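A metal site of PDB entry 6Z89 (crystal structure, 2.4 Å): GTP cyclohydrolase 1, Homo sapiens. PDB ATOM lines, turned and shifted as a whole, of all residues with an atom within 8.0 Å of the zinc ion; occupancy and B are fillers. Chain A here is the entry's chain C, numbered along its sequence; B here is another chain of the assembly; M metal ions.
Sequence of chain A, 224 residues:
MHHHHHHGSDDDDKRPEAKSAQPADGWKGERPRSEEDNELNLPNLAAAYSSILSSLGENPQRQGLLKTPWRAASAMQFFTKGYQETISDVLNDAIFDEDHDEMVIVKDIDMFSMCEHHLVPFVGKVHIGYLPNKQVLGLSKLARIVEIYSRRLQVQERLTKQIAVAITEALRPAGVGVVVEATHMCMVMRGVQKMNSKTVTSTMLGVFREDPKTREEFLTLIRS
Three residues have an atom within 4 Å of the zinc ion: Cys 115, His 118 and Cys 186.
The zinc ion is bound by a ring nitrogen (ND1) of His 118, the side-chain sulfur (SG) of Cys 186 and the side-chain sulfur (SG) of Cys 115.
The zinc ion has three donor atoms within binding distance.
The backbone carbonyl oxygen of Cys 186 is in hydrogen-bond range of the side-chain hydroxyl of Ser 140 of chain B (3.4 Å).
The side-chain sulfur (SG) of Cys 115 sits close to the backbone NH (N) of His 117 (3.6 Å).
N of Cys 115 lies within hydrogen-bond range of O of Val 120.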
ATOM      1  N   MET A 114      34.426 -23.529  -6.277  1.00  0.00           N
ATOM      2  CA  MET A 114      33.455 -23.182  -7.316  1.00  0.00           C
ATOM      3  C   MET A 114      32.315 -24.207  -7.343  1.00  0.00           C
ATOM      4  O   MET A 114      32.602 -25.393  -7.389  1.00  0.00           O
ATOM      5  CB  MET A 114      34.124 -23.166  -8.691  1.00  0.00           C
ATOM      6  CG  MET A 114      34.963 -21.947  -8.941  1.00  0.00           C
ATOM      7  SD  MET A 114      33.984 -20.488  -9.365  1.00  0.00           S
ATOM      8  CE  MET A 114      35.321 -19.336  -9.751  1.00  0.00           C
ATOM      9  N   CYS A 115      31.058 -23.765  -7.342  1.00  0.00           N
ATOM     10  CA  CYS A 115      29.927 -24.692  -7.431  1.00  0.00           C
ATOM     11  C   CYS A 115      29.827 -25.173  -8.884  1.00  0.00           C
ATOM     12  O   CYS A 115      29.679 -24.361  -9.799  1.00  0.00           O
ATOM     13  CB  CYS A 115      28.620 -24.048  -6.960  1.00  0.00           C
ATOM     14  SG  CYS A 115      27.127 -24.978  -7.381  1.00  0.00           S
ATOM     15  N   GLU A 116      29.906 -26.493  -9.101  1.00  0.00           N
ATOM     16  CA  GLU A 116      29.858 -27.052 -10.445  1.00  0.00           C
ATOM     17  C   GLU A 116      28.491 -26.871 -11.117  1.00  0.00           C
ATOM     18  O   GLU A 116      28.458 -26.575 -12.304  1.00  0.00           O
ATOM     19  CB  GLU A 116      30.297 -28.535 -10.450  1.00  0.00           C
ATOM     20  CG  GLU A 116      29.433 -29.447  -9.606  1.00  0.00           C
ATOM     21  CD  GLU A 116      29.786 -30.925  -9.667  1.00  0.00           C
ATOM     22  OE1 GLU A 116      28.920 -31.755  -9.335  1.00  0.00           O
ATOM     23  OE2 GLU A 116      30.939 -31.240 -10.058  1.00  0.00           O
ATOM     24  N   HIS A 117      27.385 -26.983 -10.363  1.00  0.00           N
ATOM     25  CA  HIS A 117      26.062 -26.852 -10.950  1.00  0.00           C
ATOM     26  C   HIS A 117      25.835 -25.551 -11.669  1.00  0.00           C
ATOM     27  O   HIS A 117      25.278 -25.581 -12.772  1.00  0.00           O
ATOM     28  CB  HIS A 117      24.954 -27.115  -9.917  1.00  0.00           C
ATOM     29  CG  HIS A 117      24.956 -28.500  -9.375  1.00  0.00           C
ATOM     30  ND1 HIS A 117      24.451 -28.786  -8.132  1.00  0.00           N
ATOM     31  CD2 HIS A 117      25.423 -29.657  -9.926  1.00  0.00           C
ATOM     32  CE1 HIS A 117      24.628 -30.083  -7.955  1.00  0.00           C
ATOM     33  NE2 HIS A 117      25.200 -30.647  -9.005  1.00  0.00           N
ATOM     34  N   HIS A 118      26.210 -24.403 -11.083  1.00  0.00           N
ATOM     35  CA  HIS A 118      25.945 -23.112 -11.724  1.00  0.00           C
ATOM     36  C   HIS A 118      27.153 -22.274 -12.105  1.00  0.00           C
ATOM     37  O   HIS A 118      26.973 -21.177 -12.628  1.00  0.00           O
ATOM     38  CB  HIS A 118      25.013 -22.263 -10.858  1.00  0.00           C
ATOM     39  CG  HIS A 118      23.786 -22.983 -10.394  1.00  0.00           C
ATOM     40  ND1 HIS A 118      23.756 -23.626  -9.171  1.00  0.00           N
ATOM     41  CD2 HIS A 118      22.583 -23.117 -10.990  1.00  0.00           C
ATOM     42  CE1 HIS A 118      22.546 -24.146  -9.071  1.00  0.00           C
ATOM     43  NE2 HIS A 118      21.797 -23.865 -10.144  1.00  0.00           N
ATOM     44  N   LEU A 119      28.371 -22.790 -11.876  1.00  0.00           N
ATOM     45  CA  LEU A 119      29.630 -22.090 -12.152  1.00  0.00           C
ATOM     46  C   LEU A 119      29.770 -20.798 -11.315  1.00  0.00           C
ATOM     47  O   LEU A 119      30.378 -19.833 -11.779  1.00  0.00           O
ATOM     48  CB  LEU A 119      29.817 -21.816 -13.653  1.00  0.00           C
ATOM     49  CG  LEU A 119      31.235 -22.083 -14.205  1.00  0.00           C
ATOM     50  CD1 LEU A 119      31.676 -23.531 -13.984  1.00  0.00           C
ATOM     51  CD2 LEU A 119      31.312 -21.779 -15.701  1.00  0.00           C
ATOM     52  N   VAL A 120      29.230 -20.787 -10.093  1.00  0.00           N
ATOM     53  CA  VAL A 120      29.304 -19.617  -9.220  1.00  0.00           C
ATOM     54  C   VAL A 120      30.085 -20.016  -7.950  1.00  0.00           C
ATOM     55  O   VAL A 120      29.944 -21.144  -7.492  1.00  0.00           O
ATOM     56  CB  VAL A 120      27.897 -19.034  -8.921  1.00  0.00           C
ATOM     57  CG1 VAL A 120      27.217 -18.550 -10.200  1.00  0.00           C
ATOM     58  CG2 VAL A 120      27.010 -20.013  -8.171  1.00  0.00           C
ATOM     59  N   PRO A 121      30.940 -19.135  -7.395  1.00  0.00           N
ATOM     60  CA  PRO A 121      31.746 -19.546  -6.227  1.00  0.00           C
ATOM     61  C   PRO A 121      30.973 -19.768  -4.953  1.00  0.00           C
ATOM     62  O   PRO A 121      29.865 -19.270  -4.789  1.00  0.00           O
ATOM     63  CB  PRO A 121      32.761 -18.414  -6.050  1.00  0.00           C
ATOM     64  CG  PRO A 121      32.675 -17.576  -7.303  1.00  0.00           C
ATOM     65  CD  PRO A 121      31.284 -17.757  -7.824  1.00  0.00           C
ATOM     66  N   PHE A 122      31.557 -20.534  -4.043  1.00  0.00           N
ATOM     67  CA  PHE A 122      31.057 -20.779  -2.698  1.00  0.00           C
ATOM     68  C   PHE A 122      32.266 -20.690  -1.771  1.00  0.00           C
ATOM     69  O   PHE A 122      33.310 -21.265  -2.034  1.00  0.00           O
ATOM     70  CB  PHE A 122      30.196 -22.051  -2.580  1.00  0.00           C
ATOM     71  CG  PHE A 122      30.849 -23.406  -2.605  1.00  0.00           C
ATOM     72  CD1 PHE A 122      30.839 -24.174  -3.754  1.00  0.00           C
ATOM     73  CD2 PHE A 122      31.345 -23.981  -1.439  1.00  0.00           C
ATOM     74  CE1 PHE A 122      31.402 -25.452  -3.766  1.00  0.00           C
ATOM     75  CE2 PHE A 122      31.893 -25.254  -1.458  1.00  0.00           C
ATOM     76  CZ  PHE A 122      31.915 -25.978  -2.613  1.00  0.00           C
ATOM     77  N   GLN A 154      33.348 -28.090  -7.867  1.00  0.00           N
ATOM     78  CA  GLN A 154      32.960 -28.985  -6.792  1.00  0.00           C
ATOM     79  C   GLN A 154      31.490 -28.935  -6.363  1.00  0.00           C
ATOM     80  O   GLN A 154      30.732 -28.075  -6.804  1.00  0.00           O
ATOM     81  CB  GLN A 154      33.811 -28.577  -5.562  1.00  0.00           C
ATOM     82  CG  GLN A 154      35.226 -29.110  -5.560  1.00  0.00           C
ATOM     83  CD  GLN A 154      35.325 -30.499  -4.984  1.00  0.00           C
ATOM     84  OE1 GLN A 154      34.328 -31.143  -4.607  1.00  0.00           O
ATOM     85  NE2 GLN A 154      36.547 -30.995  -4.918  1.00  0.00           N
ATOM     86  N   VAL A 155      31.126 -29.866  -5.466  1.00  0.00           N
ATOM     87  CA  VAL A 155      29.879 -29.954  -4.702  1.00  0.00           C
ATOM     88  C   VAL A 155      30.387 -30.070  -3.237  1.00  0.00           C
ATOM     89  O   VAL A 155      31.341 -30.823  -2.962  1.00  0.00           O
ATOM     90  CB  VAL A 155      28.940 -31.083  -5.193  1.00  0.00           C
ATOM     91  CG1 VAL A 155      29.138 -32.389  -4.440  1.00  0.00           C
ATOM     92  CG2 VAL A 155      27.495 -30.655  -5.183  1.00  0.00           C
ATOM     93  N   HIS A 184      26.852 -20.164  -0.312  1.00  0.00           N
ATOM     94  CA  HIS A 184      26.812 -20.389  -1.750  1.00  0.00           C
ATOM     95  C   HIS A 184      26.313 -19.159  -2.467  1.00  0.00           C
ATOM     96  O   HIS A 184      25.245 -18.657  -2.132  1.00  0.00           O
ATOM     97  CB  HIS A 184      25.965 -21.620  -2.062  1.00  0.00           C
ATOM     98  CG  HIS A 184      26.652 -22.880  -1.656  1.00  0.00           C
ATOM     99  ND1 HIS A 184      27.099 -23.776  -2.602  1.00  0.00           N
ATOM    100  CD2 HIS A 184      26.981 -23.322  -0.420  1.00  0.00           C
ATOM    101  CE1 HIS A 184      27.669 -24.753  -1.914  1.00  0.00           C
ATOM    102  NE2 HIS A 184      27.621 -24.527  -0.596  1.00  0.00           N
ATOM    103  N   MET A 185      27.098 -18.657  -3.441  1.00  0.00           N
ATOM    104  CA  MET A 185      26.696 -17.455  -4.160  1.00  0.00           C
ATOM    105  C   MET A 185      25.439 -17.655  -5.011  1.00  0.00           C
ATOM    106  O   MET A 185      24.844 -16.653  -5.419  1.00  0.00           O
ATOM    107  CB  MET A 185      27.839 -16.858  -4.979  1.00  0.00           C
ATOM    108  CG  MET A 185      28.982 -16.364  -4.126  1.00  0.00           C
ATOM    109  SD  MET A 185      28.541 -15.045  -2.961  1.00  0.00           S
ATOM    110  CE  MET A 185      29.075 -15.774  -1.441  1.00  0.00           C
ATOM    111  N   CYS A 186      24.968 -18.907  -5.228  1.00  0.00           N
ATOM    112  CA  CYS A 186      23.687 -19.113  -5.920  1.00  0.00           C
ATOM    113  C   CYS A 186      22.536 -19.163  -4.883  1.00  0.00           C
ATOM    114  O   CYS A 186      21.566 -19.900  -5.094  1.00  0.00           O
ATOM    115  CB  CYS A 186      23.700 -20.353  -6.793  1.00  0.00           C
ATOM    116  SG  CYS A 186      24.008 -21.894  -5.894  1.00  0.00           S
ATOM    117  N   MET A 187      22.659 -18.392  -3.765  1.00  0.00           N
ATOM    118  CA  MET A 187      21.686 -18.250  -2.675  1.00  0.00           C
ATOM    119  C   MET A 187      21.618 -16.769  -2.196  1.00  0.00           C
ATOM    120  O   MET A 187      22.345 -15.889  -2.669  1.00  0.00           O
ATOM    121  CB  MET A 187      22.025 -19.166  -1.475  1.00  0.00           C
ATOM    122  CG  MET A 187      22.158 -20.649  -1.831  1.00  0.00           C
ATOM    123  SD  MET A 187      20.669 -21.672  -1.597  1.00  0.00           S
ATOM    124  CE  MET A 187      20.347 -21.362   0.121  1.00  0.00           C
ATOM    125  N   GLY B 138      19.733 -30.758  -4.768  1.00  0.00           N
ATOM    126  CA  GLY B 138      20.404 -29.520  -5.151  1.00  0.00           C
ATOM    127  C   GLY B 138      19.998 -28.359  -4.246  1.00  0.00           C
ATOM    128  O   GLY B 138      18.822 -28.225  -3.892  1.00  0.00           O
ATOM    129  N   LEU B 139      20.943 -27.542  -3.815  1.00  0.00           N
ATOM    130  CA  LEU B 139      20.717 -26.428  -2.891  1.00  0.00           C
ATOM    131  C   LEU B 139      19.602 -25.473  -3.331  1.00  0.00           C
ATOM    132  O   LEU B 139      18.746 -25.115  -2.515  1.00  0.00           O
ATOM    133  CB  LEU B 139      22.026 -25.659  -2.702  1.00  0.00           C
ATOM    134  CG  LEU B 139      22.725 -25.793  -1.359  1.00  0.00           C
ATOM    135  CD1 LEU B 139      21.949 -25.077  -0.290  1.00  0.00           C
ATOM    136  CD2 LEU B 139      23.022 -27.241  -0.987  1.00  0.00           C
ATOM    137  N   SER B 140      19.611 -25.076  -4.606  1.00  0.00           N
ATOM    138  CA  SER B 140      18.594 -24.174  -5.117  1.00  0.00           C
ATOM    139  C   SER B 140      17.205 -24.851  -5.104  1.00  0.00           C
ATOM    140  O   SER B 140      16.216 -24.171  -4.848  1.00  0.00           O
ATOM    141  CB  SER B 140      18.967 -23.653  -6.502  1.00  0.00           C
ATOM    142  OG  SER B 140      19.768 -22.478  -6.392  1.00  0.00           O
HETATM  143 ZN    ZN M   1      24.767 -23.724  -7.396  1.00  0.00          ZN
